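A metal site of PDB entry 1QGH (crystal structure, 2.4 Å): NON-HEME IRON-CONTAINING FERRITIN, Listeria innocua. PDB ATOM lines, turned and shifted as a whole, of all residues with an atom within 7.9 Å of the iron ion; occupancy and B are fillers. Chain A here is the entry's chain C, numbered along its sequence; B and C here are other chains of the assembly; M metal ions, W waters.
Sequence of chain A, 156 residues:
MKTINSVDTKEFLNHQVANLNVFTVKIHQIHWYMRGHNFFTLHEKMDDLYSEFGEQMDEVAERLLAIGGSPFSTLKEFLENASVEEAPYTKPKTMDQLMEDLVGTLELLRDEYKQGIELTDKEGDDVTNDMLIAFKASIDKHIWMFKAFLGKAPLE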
ATOM      1  N   GLY A  54      16.402 -12.964 -17.996  1.00  0.00           N
ATOM      2  CA  GLY A  54      14.967 -13.212 -17.948  1.00  0.00           C
ATOM      3  C   GLY A  54      14.752 -14.582 -17.282  1.00  0.00           C
ATOM      4  O   GLY A  54      13.795 -14.808 -16.568  1.00  0.00           O
ATOM      5  N   GLU A  55      15.664 -15.535 -17.470  1.00  0.00           N
ATOM      6  CA  GLU A  55      15.490 -16.791 -16.760  1.00  0.00           C
ATOM      7  C   GLU A  55      15.846 -16.622 -15.279  1.00  0.00           C
ATOM      8  O   GLU A  55      15.170 -17.240 -14.450  1.00  0.00           O
ATOM      9  CB  GLU A  55      16.390 -17.894 -17.331  1.00  0.00           C
ATOM     10  CG  GLU A  55      15.931 -18.519 -18.622  1.00  0.00           C
ATOM     11  N   MET A  57      15.353 -14.146 -13.543  1.00  0.00           N
ATOM     12  CA  MET A  57      14.153 -13.494 -13.053  1.00  0.00           C
ATOM     13  C   MET A  57      13.047 -14.488 -12.746  1.00  0.00           C
ATOM     14  O   MET A  57      12.521 -14.503 -11.629  1.00  0.00           O
ATOM     15  CB  MET A  57      13.728 -12.405 -14.026  1.00  0.00           C
ATOM     16  CG  MET A  57      12.787 -11.343 -13.486  1.00  0.00           C
ATOM     17  SD  MET A  57      11.091 -11.848 -13.674  1.00  0.00           S
ATOM     18  CE  MET A  57      10.803 -11.725 -15.387  1.00  0.00           C
ATOM     19  N   ASP A  58      12.714 -15.345 -13.694  1.00  0.00           N
ATOM     20  CA  ASP A  58      11.626 -16.285 -13.416  1.00  0.00           C
ATOM     21  C   ASP A  58      11.969 -17.234 -12.276  1.00  0.00           C
ATOM     22  O   ASP A  58      11.135 -17.644 -11.466  1.00  0.00           O
ATOM     23  CB  ASP A  58      11.224 -17.076 -14.662  1.00  0.00           C
ATOM     24  CG  ASP A  58       9.828 -17.756 -14.534  1.00  0.00           C
ATOM     25  OD1 ASP A  58       8.826 -17.075 -14.195  1.00  0.00           O
ATOM     26  OD2 ASP A  58       9.720 -18.977 -14.839  1.00  0.00           O
ATOM     27  N   GLU A  59      13.247 -17.590 -12.213  1.00  0.00           N
ATOM     28  CA  GLU A  59      13.742 -18.467 -11.148  1.00  0.00           C
ATOM     29  C   GLU A  59      13.633 -17.843  -9.773  1.00  0.00           C
ATOM     30  O   GLU A  59      13.235 -18.459  -8.812  1.00  0.00           O
ATOM     31  CB  GLU A  59      15.202 -18.912 -11.356  1.00  0.00           C
ATOM     32  CG  GLU A  59      15.400 -19.906 -12.481  1.00  0.00           C
ATOM     33  N   ALA A  61      11.723 -15.406  -8.928  1.00  0.00           N
ATOM     34  CA  ALA A  61      10.311 -15.279  -8.569  1.00  0.00           C
ATOM     35  C   ALA A  61       9.730 -16.633  -8.154  1.00  0.00           C
ATOM     36  O   ALA A  61       8.932 -16.724  -7.226  1.00  0.00           O
ATOM     37  CB  ALA A  61       9.544 -14.670  -9.725  1.00  0.00           C
ATOM     38  N   GLU A  62      10.131 -17.698  -8.841  1.00  0.00           N
ATOM     39  CA  GLU A  62       9.569 -18.985  -8.507  1.00  0.00           C
ATOM     40  C   GLU A  62      10.140 -19.521  -7.209  1.00  0.00           C
ATOM     41  O   GLU A  62       9.448 -20.220  -6.483  1.00  0.00           O
ATOM     42  CB  GLU A  62       9.558 -19.961  -9.687  1.00  0.00           C
ATOM     43  CG  GLU A  62       8.619 -19.503 -10.809  1.00  0.00           C
ATOM     44  CD  GLU A  62       8.607 -20.350 -12.061  1.00  0.00           C
ATOM     45  OE1 GLU A  62       9.456 -21.272 -12.158  1.00  0.00           O
ATOM     46  OE2 GLU A  62       7.779 -20.031 -12.947  1.00  0.00           O
ATOM     47  N   LEU A  65       8.146 -17.756  -4.547  1.00  0.00           N
ATOM     48  CA  LEU A  65       6.822 -18.369  -4.457  1.00  0.00           C
ATOM     49  C   LEU A  65       6.958 -19.660  -3.648  1.00  0.00           C
ATOM     50  O   LEU A  65       6.181 -19.979  -2.745  1.00  0.00           O
ATOM     51  CB  LEU A  65       6.504 -18.658  -5.895  1.00  0.00           C
ATOM     52  CG  LEU A  65       5.191 -18.416  -6.594  1.00  0.00           C
ATOM     53  CD1 LEU A  65       4.596 -17.158  -6.051  1.00  0.00           C
ATOM     54  CD2 LEU A  65       5.650 -18.093  -7.970  1.00  0.00           C
ATOM     55  N   HIS B  28       3.373 -13.266 -16.930  1.00  0.00           N
ATOM     56  CA  HIS B  28       4.120 -13.808 -15.796  1.00  0.00           C
ATOM     57  C   HIS B  28       3.283 -13.843 -14.519  1.00  0.00           C
ATOM     58  O   HIS B  28       3.291 -14.796 -13.756  1.00  0.00           O
ATOM     59  CB  HIS B  28       5.352 -12.978 -15.531  1.00  0.00           C
ATOM     60  CG  HIS B  28       6.555 -13.485 -16.237  1.00  0.00           C
ATOM     61  ND1 HIS B  28       6.696 -14.785 -16.622  1.00  0.00           N
ATOM     62  CD2 HIS B  28       7.734 -12.880 -16.504  1.00  0.00           C
ATOM     63  CE1 HIS B  28       7.871 -14.966 -17.188  1.00  0.00           C
ATOM     64  NE2 HIS B  28       8.537 -13.826 -17.111  1.00  0.00           N
ATOM     65  N   HIS B  31       1.036 -16.614 -14.465  1.00  0.00           N
ATOM     66  CA  HIS B  31       1.831 -17.794 -14.480  1.00  0.00           C
ATOM     67  C   HIS B  31       2.383 -18.158 -13.142  1.00  0.00           C
ATOM     68  O   HIS B  31       2.523 -19.370 -12.769  1.00  0.00           O
ATOM     69  CB  HIS B  31       2.960 -17.475 -15.406  1.00  0.00           C
ATOM     70  CG  HIS B  31       4.110 -18.424 -15.331  1.00  0.00           C
ATOM     71  ND1 HIS B  31       4.067 -19.648 -15.944  1.00  0.00           N
ATOM     72  CD2 HIS B  31       5.421 -18.213 -14.976  1.00  0.00           C
ATOM     73  CE1 HIS B  31       5.243 -20.227 -15.885  1.00  0.00           C
ATOM     74  NE2 HIS B  31       6.091 -19.384 -15.264  1.00  0.00           N
ATOM     75  N   TRP B  32       2.591 -17.111 -12.330  1.00  0.00           N
ATOM     76  CA  TRP B  32       3.182 -17.349 -11.020  1.00  0.00           C
ATOM     77  C   TRP B  32       2.060 -17.598 -10.009  1.00  0.00           C
ATOM     78  O   TRP B  32       2.121 -18.431  -9.133  1.00  0.00           O
ATOM     79  CB  TRP B  32       3.901 -16.053 -10.639  1.00  0.00           C
ATOM     80  CG  TRP B  32       5.241 -15.831 -11.300  1.00  0.00           C
ATOM     81  CD1 TRP B  32       6.046 -16.782 -11.866  1.00  0.00           C
ATOM     82  CD2 TRP B  32       5.863 -14.571 -11.592  1.00  0.00           C
ATOM     83  NE1 TRP B  32       7.170 -16.230 -12.393  1.00  0.00           N
ATOM     84  CE2 TRP B  32       7.084 -14.851 -12.230  1.00  0.00           C
ATOM     85  CE3 TRP B  32       5.547 -13.245 -11.310  1.00  0.00           C
ATOM     86  CZ2 TRP B  32       7.964 -13.853 -12.658  1.00  0.00           C
ATOM     87  CZ3 TRP B  32       6.450 -12.248 -11.733  1.00  0.00           C
ATOM     88  CH2 TRP B  32       7.626 -12.556 -12.411  1.00  0.00           C
ATOM     89  N   HIS B  43       0.156 -23.469 -16.610  1.00  0.00           N
ATOM     90  CA  HIS B  43       1.457 -22.950 -16.157  1.00  0.00           C
ATOM     91  C   HIS B  43       2.369 -22.975 -17.392  1.00  0.00           C
ATOM     92  O   HIS B  43       3.045 -22.011 -17.770  1.00  0.00           O
ATOM     93  CB  HIS B  43       2.052 -23.790 -14.959  1.00  0.00           C
ATOM     94  CG  HIS B  43       3.357 -23.261 -14.437  1.00  0.00           C
ATOM     95  ND1 HIS B  43       3.465 -22.061 -13.752  1.00  0.00           N
ATOM     96  CD2 HIS B  43       4.621 -23.743 -14.524  1.00  0.00           C
ATOM     97  CE1 HIS B  43       4.745 -21.825 -13.486  1.00  0.00           C
ATOM     98  NE2 HIS B  43       5.451 -22.848 -13.935  1.00  0.00           N
ATOM     99  N   GLU B  44       2.333 -24.119 -18.063  1.00  0.00           N
ATOM    100  CA  GLU B  44       3.134 -24.251 -19.279  1.00  0.00           C
ATOM    101  C   GLU B  44       2.652 -23.388 -20.438  1.00  0.00           C
ATOM    102  O   GLU B  44       3.453 -22.687 -21.062  1.00  0.00           O
ATOM    103  CB  GLU B  44       3.312 -25.717 -19.677  1.00  0.00           C
ATOM    104  CG  GLU B  44       3.847 -26.551 -18.510  1.00  0.00           C
ATOM    105  OE1 GLU B  44       3.178 -28.445 -19.758  1.00  0.00           O
ATOM    106  N   MET B  46       1.255 -20.493 -20.286  1.00  0.00           N
ATOM    107  CA  MET B  46       1.724 -19.137 -20.119  1.00  0.00           C
ATOM    108  C   MET B  46       3.159 -18.968 -20.518  1.00  0.00           C
ATOM    109  O   MET B  46       3.519 -17.944 -21.068  1.00  0.00           O
ATOM    110  CB  MET B  46       1.537 -18.667 -18.687  1.00  0.00           C
ATOM    111  CG  MET B  46       0.097 -18.762 -18.222  1.00  0.00           C
ATOM    112  SD  MET B  46      -1.011 -17.767 -19.278  1.00  0.00           S
ATOM    113  CE  MET B  46      -1.755 -18.922 -20.340  1.00  0.00           C
ATOM    114  N   ASP B  47       4.010 -19.956 -20.283  1.00  0.00           N
ATOM    115  CA  ASP B  47       5.414 -19.840 -20.682  1.00  0.00           C
ATOM    116  C   ASP B  47       5.496 -19.638 -22.193  1.00  0.00           C
ATOM    117  O   ASP B  47       6.276 -18.845 -22.770  1.00  0.00           O
ATOM    118  CB  ASP B  47       6.291 -21.034 -20.271  1.00  0.00           C
ATOM    119  CG  ASP B  47       7.073 -20.845 -18.971  1.00  0.00           C
ATOM    120  OD1 ASP B  47       7.045 -19.642 -18.436  1.00  0.00           O
ATOM    121  OD2 ASP B  47       7.647 -21.731 -18.440  1.00  0.00           O
ATOM    122  N   LYS C 141      10.175 -26.933  -5.403  1.00  0.00           N
ATOM    123  CA  LYS C 141       9.438 -26.448  -6.554  1.00  0.00           C
ATOM    124  C   LYS C 141       8.262 -27.364  -6.792  1.00  0.00           C
ATOM    125  O   LYS C 141       7.173 -26.864  -6.993  1.00  0.00           O
ATOM    126  CB  LYS C 141      10.343 -26.386  -7.795  1.00  0.00           C
ATOM    127  CG  LYS C 141       9.768 -25.770  -9.048  1.00  0.00           C
ATOM    128  CD  LYS C 141      10.710 -26.111 -10.191  1.00  0.00           C
ATOM    129  CE  LYS C 141      10.140 -25.753 -11.545  1.00  0.00           C
ATOM    130  N   TRP C 144       5.616 -26.650  -4.432  1.00  0.00           N
ATOM    131  CA  TRP C 144       4.780 -25.495  -4.796  1.00  0.00           C
ATOM    132  C   TRP C 144       3.749 -25.840  -5.904  1.00  0.00           C
ATOM    133  O   TRP C 144       2.553 -25.544  -5.783  1.00  0.00           O
ATOM    134  CB  TRP C 144       5.688 -24.336  -5.223  1.00  0.00           C
ATOM    135  CG  TRP C 144       5.033 -23.387  -6.224  1.00  0.00           C
ATOM    136  CD1 TRP C 144       3.884 -22.682  -6.034  1.00  0.00           C
ATOM    137  CD2 TRP C 144       5.513 -23.041  -7.535  1.00  0.00           C
ATOM    138  NE1 TRP C 144       3.629 -21.885  -7.146  1.00  0.00           N
ATOM    139  CE2 TRP C 144       4.606 -22.085  -8.052  1.00  0.00           C
ATOM    140  CE3 TRP C 144       6.606 -23.447  -8.301  1.00  0.00           C
ATOM    141  CZ2 TRP C 144       4.741 -21.539  -9.327  1.00  0.00           C
ATOM    142  CZ3 TRP C 144       6.746 -22.893  -9.578  1.00  0.00           C
ATOM    143  CH2 TRP C 144       5.815 -21.963 -10.058  1.00  0.00           C
HETATM  144 FE    FE M   1       8.348 -20.087 -15.035  1.00  0.00          FE
HETATM  145  O   HOH W   1       7.901 -23.144 -14.051  1.00  0.00           O
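Water W1 lies within hydrogen-bond range of NE2 of His 43 of chain B (2.5 Å) and OE1 of Glu 62 (3.1 Å).
A ring nitrogen (ND1) of His 43 of chain B sits at hydrogen-bond distance from the backbone carbonyl oxygen (O) of His 31 of chain B (3.0 Å). NE1 of Trp 32 of chain B sits at hydrogen-bond distance from OD1 of Asp 58, 2.6 Å away. NE2 of His 31 of chain B lies close to OD1 of Asp 47 of chain B, at 3.3 Å.
The iron ion is bound by the side-chain carboxylate of Asp 58 (1.8 Å), the side-chain carboxylate of Glu 62 (2.2 Å) and a ring nitrogen (NE2) of His 31 of chain B (2.4 Å). The iron ion has three donor atoms within binding distance.
Asp 47 of chain B touches the iron ion (OD1 to FE, 3.7 Å). The nearest printed residue that does not touch the iron ion is His 43 of chain B (4.2 Å).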
